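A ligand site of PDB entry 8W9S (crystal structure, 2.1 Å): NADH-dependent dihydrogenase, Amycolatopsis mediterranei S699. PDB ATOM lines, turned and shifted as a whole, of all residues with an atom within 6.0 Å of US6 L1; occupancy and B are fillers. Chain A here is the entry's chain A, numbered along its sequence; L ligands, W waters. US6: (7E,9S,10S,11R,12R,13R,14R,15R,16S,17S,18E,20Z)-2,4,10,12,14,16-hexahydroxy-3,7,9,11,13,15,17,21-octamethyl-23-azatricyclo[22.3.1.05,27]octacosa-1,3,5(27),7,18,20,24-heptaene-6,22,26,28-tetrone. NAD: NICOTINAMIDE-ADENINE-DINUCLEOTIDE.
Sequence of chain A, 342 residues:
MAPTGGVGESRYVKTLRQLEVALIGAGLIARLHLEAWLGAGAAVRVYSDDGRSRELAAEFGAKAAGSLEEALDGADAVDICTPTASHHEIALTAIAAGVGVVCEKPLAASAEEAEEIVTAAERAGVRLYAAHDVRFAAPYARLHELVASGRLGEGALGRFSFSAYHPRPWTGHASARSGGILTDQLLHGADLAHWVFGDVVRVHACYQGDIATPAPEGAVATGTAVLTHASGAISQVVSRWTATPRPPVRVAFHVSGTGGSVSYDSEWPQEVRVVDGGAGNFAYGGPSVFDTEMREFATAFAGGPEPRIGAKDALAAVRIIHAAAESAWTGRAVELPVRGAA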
ATOM      1  N   LEU A  28       2.892  -3.132  23.451  1.00  0.00           N
ATOM      2  CA  LEU A  28       3.803  -4.065  24.126  1.00  0.00           C
ATOM      3  C   LEU A  28       5.133  -3.417  24.472  1.00  0.00           C
ATOM      4  O   LEU A  28       5.653  -3.610  25.579  1.00  0.00           O
ATOM      5  CB  LEU A  28       3.982  -5.321  23.278  1.00  0.00           C
ATOM      6  CG  LEU A  28       4.967  -6.355  23.816  1.00  0.00           C
ATOM      7  CD1 LEU A  28       4.614  -6.771  25.237  1.00  0.00           C
ATOM      8  CD2 LEU A  28       4.851  -7.573  22.901  1.00  0.00           C
ATOM      9  N   ILE A  29       5.696  -2.609  23.564  1.00  0.00           N
ATOM     10  CA  ILE A  29       6.965  -1.936  23.847  1.00  0.00           C
ATOM     11  C   ILE A  29       6.787  -0.920  24.965  1.00  0.00           C
ATOM     12  O   ILE A  29       7.584  -0.884  25.911  1.00  0.00           O
ATOM     13  CB  ILE A  29       7.537  -1.286  22.573  1.00  0.00           C
ATOM     14  CG1 ILE A  29       7.978  -2.341  21.596  1.00  0.00           C
ATOM     15  CG2 ILE A  29       8.791  -0.457  22.890  1.00  0.00           C
ATOM     16  CD1 ILE A  29       9.133  -3.167  22.125  1.00  0.00           C
ATOM     17  N   LEU A  32       6.751  -2.498  28.235  1.00  0.00           N
ATOM     18  CA  LEU A  32       8.082  -2.921  28.671  1.00  0.00           C
ATOM     19  C   LEU A  32       8.924  -1.732  29.092  1.00  0.00           C
ATOM     20  O   LEU A  32       9.673  -1.796  30.071  1.00  0.00           O
ATOM     21  CB  LEU A  32       8.770  -3.692  27.545  1.00  0.00           C
ATOM     22  CG  LEU A  32       8.155  -5.057  27.237  1.00  0.00           C
ATOM     23  CD1 LEU A  32       8.554  -5.501  25.839  1.00  0.00           C
ATOM     24  CD2 LEU A  32       8.584  -6.088  28.269  1.00  0.00           C
ATOM     25  N   ASP A 133      18.046  -1.790  21.000  1.00  0.00           N
ATOM     26  CA  ASP A 133      18.181  -2.658  22.170  1.00  0.00           C
ATOM     27  C   ASP A 133      19.402  -3.568  22.105  1.00  0.00           C
ATOM     28  O   ASP A 133      19.959  -3.925  23.143  1.00  0.00           O
ATOM     29  CB  ASP A 133      16.932  -3.533  22.343  1.00  0.00           C
ATOM     30  CG  ASP A 133      15.632  -2.757  22.221  1.00  0.00           C
ATOM     31  OD1 ASP A 133      14.792  -3.165  21.388  1.00  0.00           O
ATOM     32  OD2 ASP A 133      15.431  -1.754  22.929  1.00  0.00           O
ATOM     33  N   VAL A 134      19.813  -3.978  20.897  1.00  0.00           N
ATOM     34  CA  VAL A 134      20.919  -4.930  20.764  1.00  0.00           C
ATOM     35  C   VAL A 134      22.166  -4.422  21.458  1.00  0.00           C
ATOM     36  O   VAL A 134      22.913  -5.209  22.060  1.00  0.00           O
ATOM     37  CB  VAL A 134      21.192  -5.278  19.278  1.00  0.00           C
ATOM     38  CG1 VAL A 134      21.603  -4.038  18.458  1.00  0.00           C
ATOM     39  CG2 VAL A 134      22.286  -6.331  19.167  1.00  0.00           C
ATOM     40  N   ALA A 137      22.638  -5.575  25.362  1.00  0.00           N
ATOM     41  CA  ALA A 137      22.831  -6.947  25.793  1.00  0.00           C
ATOM     42  C   ALA A 137      24.311  -7.319  25.747  1.00  0.00           C
ATOM     43  O   ALA A 137      25.052  -6.840  24.891  1.00  0.00           O
ATOM     44  CB  ALA A 137      22.017  -7.923  24.938  1.00  0.00           C
ATOM     45  N   TYR A 140      26.862  -8.379  22.566  1.00  0.00           N
ATOM     46  CA  TYR A 140      27.094  -7.306  21.603  1.00  0.00           C
ATOM     47  C   TYR A 140      27.872  -6.148  22.204  1.00  0.00           C
ATOM     48  O   TYR A 140      28.799  -5.622  21.583  1.00  0.00           O
ATOM     49  CB  TYR A 140      25.740  -6.837  21.038  1.00  0.00           C
ATOM     50  CG  TYR A 140      24.823  -8.017  20.842  1.00  0.00           C
ATOM     51  CD1 TYR A 140      25.022  -8.917  19.790  1.00  0.00           C
ATOM     52  CD2 TYR A 140      23.811  -8.268  21.734  1.00  0.00           C
ATOM     53  CE1 TYR A 140      24.207 -10.019  19.636  1.00  0.00           C
ATOM     54  CE2 TYR A 140      22.995  -9.372  21.597  1.00  0.00           C
ATOM     55  CZ  TYR A 140      23.193 -10.247  20.549  1.00  0.00           C
ATOM     56  OH  TYR A 140      22.355 -11.342  20.430  1.00  0.00           O
ATOM     57  N   PHE A 162      20.299 -12.576  12.565  1.00  0.00           N
ATOM     58  CA  PHE A 162      19.213 -12.359  13.512  1.00  0.00           C
ATOM     59  C   PHE A 162      17.987 -13.066  12.954  1.00  0.00           C
ATOM     60  O   PHE A 162      17.542 -12.766  11.840  1.00  0.00           O
ATOM     61  CB  PHE A 162      18.930 -10.869  13.696  1.00  0.00           C
ATOM     62  CG  PHE A 162      19.973 -10.148  14.509  1.00  0.00           C
ATOM     63  CD1 PHE A 162      21.186  -9.798  13.945  1.00  0.00           C
ATOM     64  CD2 PHE A 162      19.744  -9.842  15.835  1.00  0.00           C
ATOM     65  CE1 PHE A 162      22.164  -9.163  14.699  1.00  0.00           C
ATOM     66  CE2 PHE A 162      20.707  -9.183  16.592  1.00  0.00           C
ATOM     67  CZ  PHE A 162      21.921  -8.849  16.014  1.00  0.00           C
ATOM     68  N   SER A 163      17.441 -14.001  13.721  1.00  0.00           N
ATOM     69  CA  SER A 163      16.395 -14.885  13.227  1.00  0.00           C
ATOM     70  C   SER A 163      15.366 -15.128  14.305  1.00  0.00           C
ATOM     71  O   SER A 163      15.733 -15.454  15.442  1.00  0.00           O
ATOM     72  CB  SER A 163      17.013 -16.214  12.739  1.00  0.00           C
ATOM     73  OG  SER A 163      16.015 -17.113  12.280  1.00  0.00           O
ATOM     74  N   ALA A 164      14.082 -14.987  13.979  1.00  0.00           N
ATOM     75  CA  ALA A 164      13.053 -15.125  15.000  1.00  0.00           C
ATOM     76  C   ALA A 164      11.728 -15.565  14.403  1.00  0.00           C
ATOM     77  O   ALA A 164      11.468 -15.393  13.207  1.00  0.00           O
ATOM     78  CB  ALA A 164      12.846 -13.804  15.772  1.00  0.00           C
ATOM     79  N   TYR A 165      10.897 -16.126  15.269  1.00  0.00           N
ATOM     80  CA  TYR A 165       9.487 -16.352  14.983  1.00  0.00           C
ATOM     81  C   TYR A 165       8.711 -15.119  15.430  1.00  0.00           C
ATOM     82  O   TYR A 165       8.855 -14.663  16.557  1.00  0.00           O
ATOM     83  CB  TYR A 165       8.994 -17.597  15.741  1.00  0.00           C
ATOM     84  CG  TYR A 165       7.492 -17.710  15.819  1.00  0.00           C
ATOM     85  CD1 TYR A 165       6.759 -18.154  14.719  1.00  0.00           C
ATOM     86  CD2 TYR A 165       6.796 -17.375  16.982  1.00  0.00           C
ATOM     87  CE1 TYR A 165       5.393 -18.271  14.767  1.00  0.00           C
ATOM     88  CE2 TYR A 165       5.429 -17.477  17.044  1.00  0.00           C
ATOM     89  CZ  TYR A 165       4.725 -17.926  15.922  1.00  0.00           C
ATOM     90  OH  TYR A 165       3.353 -18.029  15.954  1.00  0.00           O
ATOM     91  N   HIS A 166       7.915 -14.539  14.529  1.00  0.00           N
ATOM     92  CA  HIS A 166       7.124 -13.367  14.893  1.00  0.00           C
ATOM     93  C   HIS A 166       5.797 -13.801  15.512  1.00  0.00           C
ATOM     94  O   HIS A 166       4.935 -14.306  14.772  1.00  0.00           O
ATOM     95  CB  HIS A 166       6.877 -12.467  13.691  1.00  0.00           C
ATOM     96  CG  HIS A 166       6.461 -11.085  14.060  1.00  0.00           C
ATOM     97  ND1 HIS A 166       5.399 -10.430  13.476  1.00  0.00           N
ATOM     98  CD2 HIS A 166       6.971 -10.213  14.977  1.00  0.00           C
ATOM     99  CE1 HIS A 166       5.280  -9.226  13.995  1.00  0.00           C
ATOM    100  NE2 HIS A 166       6.215  -9.066  14.904  1.00  0.00           N
ATOM    101  N   PRO A 167       5.580 -13.612  16.820  1.00  0.00           N
ATOM    102  CA  PRO A 167       4.414 -14.215  17.463  1.00  0.00           C
ATOM    103  C   PRO A 167       3.131 -13.399  17.387  1.00  0.00           C
ATOM    104  O   PRO A 167       2.085 -13.908  17.813  1.00  0.00           O
ATOM    105  CB  PRO A 167       4.886 -14.350  18.923  1.00  0.00           C
ATOM    106  CG  PRO A 167       5.754 -13.177  19.122  1.00  0.00           C
ATOM    107  CD  PRO A 167       6.476 -12.963  17.794  1.00  0.00           C
ATOM    108  N   ARG A 168       3.180 -12.170  16.881  1.00  0.00           N
ATOM    109  CA  ARG A 168       2.022 -11.317  16.699  1.00  0.00           C
ATOM    110  C   ARG A 168       1.892 -11.014  15.215  1.00  0.00           C
ATOM    111  O   ARG A 168       2.866 -11.117  14.461  1.00  0.00           O
ATOM    112  CB  ARG A 168       2.163  -9.977  17.448  1.00  0.00           C
ATOM    113  CG  ARG A 168       2.874 -10.043  18.775  1.00  0.00           C
ATOM    114  CD  ARG A 168       2.838  -8.689  19.524  1.00  0.00           C
ATOM    115  NE  ARG A 168       3.913  -7.786  19.108  1.00  0.00           N
ATOM    116  CZ  ARG A 168       3.848  -6.456  19.144  1.00  0.00           C
ATOM    117  NH1 ARG A 168       2.739  -5.850  19.575  1.00  0.00           N
ATOM    118  NH2 ARG A 168       4.891  -5.718  18.761  1.00  0.00           N
ATOM    119  N   TRP A 170       1.606  -8.571  11.893  1.00  0.00           N
ATOM    120  CA  TRP A 170       1.931  -7.224  11.460  1.00  0.00           C
ATOM    121  C   TRP A 170       0.639  -6.596  10.961  1.00  0.00           C
ATOM    122  O   TRP A 170       0.121  -6.993   9.916  1.00  0.00           O
ATOM    123  CB  TRP A 170       2.955  -7.214  10.326  1.00  0.00           C
ATOM    124  CG  TRP A 170       4.366  -7.535  10.655  1.00  0.00           C
ATOM    125  CD1 TRP A 170       5.347  -6.649  11.036  1.00  0.00           C
ATOM    126  CD2 TRP A 170       4.975  -8.824  10.619  1.00  0.00           C
ATOM    127  NE1 TRP A 170       6.542  -7.321  11.229  1.00  0.00           N
ATOM    128  CE2 TRP A 170       6.341  -8.658  10.983  1.00  0.00           C
ATOM    129  CE3 TRP A 170       4.506 -10.107  10.321  1.00  0.00           C
ATOM    130  CZ2 TRP A 170       7.235  -9.726  11.054  1.00  0.00           C
ATOM    131  CZ3 TRP A 170       5.422 -11.187  10.392  1.00  0.00           C
ATOM    132  CH2 TRP A 170       6.766 -10.973  10.731  1.00  0.00           C
ATOM    133  N   ASP A 184      12.219  -4.684   9.560  1.00  0.00           N
ATOM    134  CA  ASP A 184      12.152  -4.799  11.027  1.00  0.00           C
ATOM    135  C   ASP A 184      13.300  -5.631  11.578  1.00  0.00           C
ATOM    136  O   ASP A 184      13.876  -5.281  12.620  1.00  0.00           O
ATOM    137  CB  ASP A 184      10.828  -5.433  11.450  1.00  0.00           C
ATOM    138  CG  ASP A 184       9.618  -4.568  11.144  1.00  0.00           C
ATOM    139  OD1 ASP A 184       9.755  -3.318  11.151  1.00  0.00           O
ATOM    140  OD2 ASP A 184       8.542  -5.141  10.916  1.00  0.00           O
ATOM    141  N   GLN A 185      13.592  -6.759  10.942  1.00  0.00           N
ATOM    142  CA  GLN A 185      14.615  -7.651  11.474  1.00  0.00           C
ATOM    143  C   GLN A 185      16.003  -7.144  11.139  1.00  0.00           C
ATOM    144  O   GLN A 185      16.954  -7.428  11.871  1.00  0.00           O
ATOM    145  CB  GLN A 185      14.409  -9.058  10.930  1.00  0.00           C
ATOM    146  CG  GLN A 185      15.253 -10.116  11.605  1.00  0.00           C
ATOM    147  CD  GLN A 185      14.729 -10.453  12.997  1.00  0.00           C
ATOM    148  OE1 GLN A 185      14.929  -9.688  13.947  1.00  0.00           O
ATOM    149  NE2 GLN A 185      14.044 -11.589  13.119  1.00  0.00           N
ATOM    150  N   HIS A 188      18.508  -4.643  13.676  1.00  0.00           N
ATOM    151  CA  HIS A 188      19.461  -5.141  14.663  1.00  0.00           C
ATOM    152  C   HIS A 188      20.836  -5.337  14.033  1.00  0.00           C
ATOM    153  O   HIS A 188      21.845  -4.819  14.514  1.00  0.00           O
ATOM    154  CB  HIS A 188      18.999  -6.471  15.278  1.00  0.00           C
ATOM    155  CG  HIS A 188      17.625  -6.420  15.845  1.00  0.00           C
ATOM    156  ND1 HIS A 188      17.273  -5.580  16.877  1.00  0.00           N
ATOM    157  CD2 HIS A 188      16.508  -7.111  15.521  1.00  0.00           C
ATOM    158  CE1 HIS A 188      15.996  -5.763  17.173  1.00  0.00           C
ATOM    159  NE2 HIS A 188      15.505  -6.681  16.356  1.00  0.00           N
ATOM    160  N   TRP A 241      12.727 -14.274   9.411  1.00  0.00           N
ATOM    161  CA  TRP A 241      11.525 -14.591  10.165  1.00  0.00           C
ATOM    162  C   TRP A 241      11.195 -16.047   9.877  1.00  0.00           C
ATOM    163  O   TRP A 241      11.221 -16.460   8.715  1.00  0.00           O
ATOM    164  CB  TRP A 241      10.368 -13.684   9.756  1.00  0.00           C
ATOM    165  CG  TRP A 241      10.573 -12.258  10.157  1.00  0.00           C
ATOM    166  CD1 TRP A 241      10.813 -11.193   9.339  1.00  0.00           C
ATOM    167  CD2 TRP A 241      10.535 -11.742  11.504  1.00  0.00           C
ATOM    168  NE1 TRP A 241      10.945 -10.034  10.097  1.00  0.00           N
ATOM    169  CE2 TRP A 241      10.779 -10.351  11.421  1.00  0.00           C
ATOM    170  CE3 TRP A 241      10.330 -12.328  12.767  1.00  0.00           C
ATOM    171  CZ2 TRP A 241      10.826  -9.538  12.560  1.00  0.00           C
ATOM    172  CZ3 TRP A 241      10.364 -11.514  13.889  1.00  0.00           C
ATOM    173  CH2 TRP A 241      10.610 -10.136  13.775  1.00  0.00           C
ATOM    174  N   VAL A 249      14.015 -17.330  19.134  1.00  0.00           N
ATOM    175  CA  VAL A 249      14.998 -16.355  18.676  1.00  0.00           C
ATOM    176  C   VAL A 249      16.342 -17.059  18.569  1.00  0.00           C
ATOM    177  O   VAL A 249      16.708 -17.849  19.445  1.00  0.00           O
ATOM    178  CB  VAL A 249      15.140 -15.159  19.648  1.00  0.00           C
ATOM    179  CG1 VAL A 249      16.216 -14.173  19.154  1.00  0.00           C
ATOM    180  CG2 VAL A 249      13.796 -14.430  19.861  1.00  0.00           C
ATOM    181  N   ARG A 250      17.111 -16.730  17.524  1.00  0.00           N
ATOM    182  CA  ARG A 250      18.533 -17.083  17.512  1.00  0.00           C
ATOM    183  C   ARG A 250      19.319 -15.942  16.896  1.00  0.00           C
ATOM    184  O   ARG A 250      18.949 -15.408  15.840  1.00  0.00           O
ATOM    185  CB  ARG A 250      18.802 -18.398  16.737  1.00  0.00           C
ATOM    186  CG  ARG A 250      20.319 -18.672  16.600  1.00  0.00           C
ATOM    187  CD  ARG A 250      20.638 -20.021  16.003  1.00  0.00           C
ATOM    188  NE  ARG A 250      22.084 -20.293  16.008  1.00  0.00           N
ATOM    189  CZ  ARG A 250      22.873 -20.119  14.958  1.00  0.00           C
ATOM    190  NH1 ARG A 250      22.345 -19.652  13.829  1.00  0.00           N
ATOM    191  NH2 ARG A 250      24.182 -20.407  15.030  1.00  0.00           N
ATOM    192  N   VAL A 251      20.424 -15.588  17.554  1.00  0.00           N
ATOM    193  CA  VAL A 251      21.409 -14.634  17.059  1.00  0.00           C
ATOM    194  C   VAL A 251      22.762 -15.317  17.066  1.00  0.00           C
ATOM    195  O   VAL A 251      23.102 -16.052  17.999  1.00  0.00           O
ATOM    196  CB  VAL A 251      21.462 -13.358  17.920  1.00  0.00           C
ATOM    197  CG1 VAL A 251      22.374 -12.295  17.265  1.00  0.00           C
ATOM    198  CG2 VAL A 251      20.051 -12.820  18.191  1.00  0.00           C
ATOM    199  N   VAL A 289      17.299  -6.140  28.813  1.00  0.00           N
ATOM    200  CA  VAL A 289      17.897  -5.063  28.041  1.00  0.00           C
ATOM    201  C   VAL A 289      17.171  -3.756  28.289  1.00  0.00           C
ATOM    202  O   VAL A 289      17.784  -2.690  28.255  1.00  0.00           O
ATOM    203  CB  VAL A 289      17.917  -5.400  26.521  1.00  0.00           C
ATOM    204  CG1 VAL A 289      18.608  -6.729  26.281  1.00  0.00           C
ATOM    205  CG2 VAL A 289      16.507  -5.392  25.942  1.00  0.00           C
ATOM    206  N   PHE A 290      15.864  -3.814  28.562  1.00  0.00           N
ATOM    207  CA  PHE A 290      15.106  -2.586  28.805  1.00  0.00           C
ATOM    208  C   PHE A 290      15.525  -1.932  30.124  1.00  0.00           C
ATOM    209  O   PHE A 290      15.602  -0.701  30.207  1.00  0.00           O
ATOM    210  CB  PHE A 290      13.615  -2.885  28.775  1.00  0.00           C
ATOM    211  CG  PHE A 290      13.128  -3.415  27.461  1.00  0.00           C
ATOM    212  CD1 PHE A 290      13.267  -2.677  26.294  1.00  0.00           C
ATOM    213  CD2 PHE A 290      12.541  -4.673  27.382  1.00  0.00           C
ATOM    214  CE1 PHE A 290      12.816  -3.167  25.074  1.00  0.00           C
ATOM    215  CE2 PHE A 290      12.084  -5.169  26.166  1.00  0.00           C
ATOM    216  CZ  PHE A 290      12.222  -4.423  25.006  1.00  0.00           C
HETATM  217  C01 US6 L   1      19.093  -8.408  22.585  1.00  0.00           C
HETATM  218  C02 US6 L   1      17.729  -8.686  21.970  1.00  0.00           C
HETATM  219  C03 US6 L   1      17.915  -9.578  20.727  1.00  0.00           C
HETATM  220  C04 US6 L   1      17.043  -9.519  19.683  1.00  0.00           C
HETATM  221  C05 US6 L   1      17.266 -10.473  18.452  1.00  0.00           C
HETATM  222  C06 US6 L   1      16.249 -10.894  17.650  1.00  0.00           C
HETATM  223  C07 US6 L   1      14.792 -10.422  17.871  1.00  0.00           C
HETATM  224  C10 US6 L   1      12.624  -9.696  16.827  1.00  0.00           C
HETATM  225  C11 US6 L   1      11.670 -10.428  17.709  1.00  0.00           C
HETATM  226  C12 US6 L   1      10.251  -9.908  17.849  1.00  0.00           C
HETATM  227  C14 US6 L   1       9.801  -8.620  17.084  1.00  0.00           C
HETATM  228  C15 US6 L   1       8.463  -8.113  17.186  1.00  0.00           C
HETATM  229  C16 US6 L   1       8.098  -6.936  16.493  1.00  0.00           C
HETATM  230  C17 US6 L   1       9.017  -6.262  15.644  1.00  0.00           C
HETATM  231  C18 US6 L   1      10.348  -6.755  15.526  1.00  0.00           C
HETATM  232  C19 US6 L   1      10.741  -7.942  16.248  1.00  0.00           C
HETATM  233  C20 US6 L   1      12.216  -8.458  16.093  1.00  0.00           C
HETATM  234  C23 US6 L   1       8.559  -4.988  14.894  1.00  0.00           C
HETATM  235  C25 US6 L   1       7.354  -8.729  18.120  1.00  0.00           C
HETATM  236  C27 US6 L   1       7.699  -8.759  19.662  1.00  0.00           C
HETATM  237  C28 US6 L   1       8.654  -7.890  20.150  1.00  0.00           C
HETATM  238  C29 US6 L   1       9.070  -7.847  21.645  1.00  0.00           C
HETATM  239  C30 US6 L   1      10.580  -7.637  21.776  1.00  0.00           C
HETATM  240  C31 US6 L   1      11.260  -8.913  22.320  1.00  0.00           C
HETATM  241  C32 US6 L   1      12.753  -8.689  22.644  1.00  0.00           C
HETATM  242  C33 US6 L   1      13.192  -9.686  23.744  1.00  0.00           C
HETATM  243  C34 US6 L   1      14.705  -9.578  24.021  1.00  0.00           C
HETATM  244  C35 US6 L   1      15.509  -9.751  22.729  1.00  0.00           C
HETATM  245  C36 US6 L   1      16.993  -9.466  23.059  1.00  0.00           C
HETATM  246  C38 US6 L   1      15.357 -11.171  22.249  1.00  0.00           C
HETATM  247  C40 US6 L   1      12.441  -9.352  25.010  1.00  0.00           C
HETATM  248  C42 US6 L   1      11.103 -10.022  21.294  1.00  0.00           C
HETATM  249  C44 US6 L   1       8.441  -6.649  22.309  1.00  0.00           C
HETATM  250  C45 US6 L   1       6.983  -9.742  20.619  1.00  0.00           C
HETATM  251  C46 US6 L   1      16.506 -11.819  16.436  1.00  0.00           C
HETATM  252  N09 US6 L   1      14.006 -10.171  16.678  1.00  0.00           N
HETATM  253  O08 US6 L   1      14.325 -10.262  18.950  1.00  0.00           O
HETATM  254  O13 US6 L   1       9.515 -10.513  18.546  1.00  0.00           O
HETATM  255  O21 US6 L   1      13.011  -7.902  15.411  1.00  0.00           O
HETATM  256  O22 US6 L   1      11.288  -6.111  14.698  1.00  0.00           O
HETATM  257  O24 US6 L   1       6.781  -6.460  16.616  1.00  0.00           O
HETATM  258  O26 US6 L   1       6.301  -9.089  17.714  1.00  0.00           O
HETATM  259  O37 US6 L   1      17.653 -10.672  23.221  1.00  0.00           O
HETATM  260  O39 US6 L   1      15.013  -8.356  24.631  1.00  0.00           O
HETATM  261  O41 US6 L   1      12.936  -7.429  23.171  1.00  0.00           O
HETATM  262  O43 US6 L   1      11.075  -7.279  20.524  1.00  0.00           O
HETATM  263  PA  NAD L   2       1.704  -1.466  19.061  1.00  0.00           P
HETATM  264  O1A NAD L   2       0.695  -1.472  17.957  1.00  0.00           O
HETATM  265  O2A NAD L   2       1.487  -2.608  20.057  1.00  0.00           O
HETATM  266  O5B NAD L   2       1.634  -0.014  19.877  1.00  0.00           O
HETATM  267  C5B NAD L   2       1.018   1.107  19.272  1.00  0.00           C
HETATM  268  C4B NAD L   2       0.564   2.045  20.456  1.00  0.00           C
HETATM  269  O4B NAD L   2       0.766   3.296  20.134  1.00  0.00           O
HETATM  270  C3B NAD L   2      -1.006   1.870  20.657  1.00  0.00           C
HETATM  271  O3B NAD L   2      -1.294   1.924  22.052  1.00  0.00           O
HETATM  272  C2B NAD L   2      -1.587   3.053  19.880  1.00  0.00           C
HETATM  273  O2B NAD L   2      -2.863   3.412  20.410  1.00  0.00           O
HETATM  274  C1B NAD L   2      -0.693   4.033  20.088  1.00  0.00           C
HETATM  275  N9A NAD L   2      -0.580   5.115  19.103  1.00  0.00           N
HETATM  276  C8A NAD L   2      -0.583   4.982  17.774  1.00  0.00           C
HETATM  277  N7A NAD L   2      -0.467   6.166  17.219  1.00  0.00           N
HETATM  278  C5A NAD L   2      -0.380   7.101  18.194  1.00  0.00           C
HETATM  279  C6A NAD L   2      -0.243   8.505  18.253  1.00  0.00           C
HETATM  280  N6A NAD L   2      -0.146   9.270  17.052  1.00  0.00           N
HETATM  281  N1A NAD L   2      -0.185   9.138  19.431  1.00  0.00           N
HETATM  282  C2A NAD L   2      -0.265   8.441  20.542  1.00  0.00           C
HETATM  283  N3A NAD L   2      -0.401   7.117  20.545  1.00  0.00           N
HETATM  284  C4A NAD L   2      -0.451   6.420  19.394  1.00  0.00           C
HETATM  285  O3  NAD L   2       3.186  -1.608  18.378  1.00  0.00           O
HETATM  286  PN  NAD L   2       4.557  -1.724  19.257  1.00  0.00           P
HETATM  287  O1N NAD L   2       4.284  -1.819  20.729  1.00  0.00           O
HETATM  288  O2N NAD L   2       5.346  -2.916  18.810  1.00  0.00           O
HETATM  289  O5D NAD L   2       5.353  -0.338  18.878  1.00  0.00           O
HETATM  290  C5D NAD L   2       5.511  -0.106  17.498  1.00  0.00           C
HETATM  291  C4D NAD L   2       6.866   0.662  17.394  1.00  0.00           C
HETATM  292  O4D NAD L   2       7.771   0.056  18.122  1.00  0.00           O
HETATM  293  C3D NAD L   2       7.367   0.596  15.850  1.00  0.00           C
HETATM  294  O3D NAD L   2       8.199   1.653  15.680  1.00  0.00           O
HETATM  295  C2D NAD L   2       7.967  -0.551  15.760  1.00  0.00           C
HETATM  296  O2D NAD L   2       8.890  -0.604  14.719  1.00  0.00           O
HETATM  297  C1D NAD L   2       8.746  -0.603  17.120  1.00  0.00           C
HETATM  298  N1N NAD L   2       9.239  -1.965  17.490  1.00  0.00           N
HETATM  299  C2N NAD L   2      10.376  -2.396  16.969  1.00  0.00           C
HETATM  300  C3N NAD L   2      10.875  -3.656  17.268  1.00  0.00           C
HETATM  301  C7N NAD L   2      12.218  -4.183  16.647  1.00  0.00           C
HETATM  302  O7N NAD L   2      12.543  -3.862  15.557  1.00  0.00           O
HETATM  303  N7N NAD L   2      13.058  -5.097  17.460  1.00  0.00           N
HETATM  304  C4N NAD L   2      10.163  -4.456  18.171  1.00  0.00           C
HETATM  305  C5N NAD L   2       8.976  -3.983  18.700  1.00  0.00           C
HETATM  306  C6N NAD L   2       8.542  -2.708  18.329  1.00  0.00           C
HETATM  307  O   HOH W   1      10.303 -13.172  19.812  1.00  0.00           O
HETATM  308  O   HOH W   2      15.484  -8.294  27.316  1.00  0.00           O
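O26 of US6 L1 lies within hydrogen-bond range of NE2 of His 166, at 2.8 Å.
N09 of US6 L1 is in hydrogen-bond range of OE1 of Gln 185 (2.9 Å).
A ring nitrogen (NE2) of His 188 lies within hydrogen-bond range of an oxygen (O21) of US6 L1.
An oxygen (O24) of US6 L1 sits at hydrogen-bond distance from the guanidinium group of Arg 168, 3.0 Å away.
The backbone carbonyl oxygen (O) of Asp 184 sits close to an oxygen (O22) of US6 L1 (3.4 Å).
A nitrogen (N7N) of NAD L2 lies close to a ring nitrogen (NE2) of His 188, 3.1 Å away.
NH2 of Arg 168 is in salt-bridge range of O2N of NAD L2 (2.8 Å).
N of Ile 29 lies within hydrogen-bond range of O1N of NAD L2, at 3.3 Å.
The backbone NH (N) of Leu 28 sits at hydrogen-bond distance from an oxygen (O1N) of NAD L2.
An oxygen (O7N) of NAD L2 sits at hydrogen-bond distance from an oxygen (O22) of US6 L1 (2.7 Å).
Water W2 lies within hydrogen-bond range of an oxygen (O39) of US6 L1 (2.7 Å) and the backbone NH (N) of Val 289 (3.2 Å).
CD2 of Leu 28 touches C44 of US6 L1 (3.8 Å).
Ile 29 touches US6 L1.
CD1 of Leu 32 touches C44 of US6 L1 (3.7 Å).
Ala 137 touches US6 L1 (CB to C01, 3.8 Å).
Phe 162 touches US6 L1.
Ser 163 touches US6 L1.
Ala 164 touches US6 L1 (CB to N09, 3.9 Å).
Pro 167 touches US6 L1 (CD to O26, 3.9 Å).
Trp 241 touches US6 L1.
CG1 of Val 249 touches C46 of US6 L1, at 3.6 Å.
Val 251 touches US6 L1 (CG2 to C05, 3.7 Å).
Val 289 touches US6 L1 (CG2 to O39, 3.6 Å).
Phe 290 touches US6 L1 (CZ to O41, 3.6 Å).
Hydrophobic or aromatic side chains within 4 Å of US6 L1: Leu 28, Ile 29, Leu 32, Ala 137, Phe 162, Ala 164, His 166, Pro 167, His 188, Trp 241, Val 249, Val 251, Val 289 and Phe 290.
Of the 24 residues printed, 18 come within 4 Å of US6 L1.
The nearest printed residue that does not touch US6 L1 is Tyr 140 (4.1 Å).
The backbone carbonyl oxygen of Arg 168 is in hydrogen-bond range of a ring nitrogen (ND1) of His 166, 2.8 Å away.
OD2 of Asp 184 sits at hydrogen-bond distance from NE1 of Trp 170, at 3.0 Å.
The backbone carbonyl oxygen (O) of Ser 163 is in hydrogen-bond range of the backbone NH (N) of Arg 250, at 2.8 Å.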
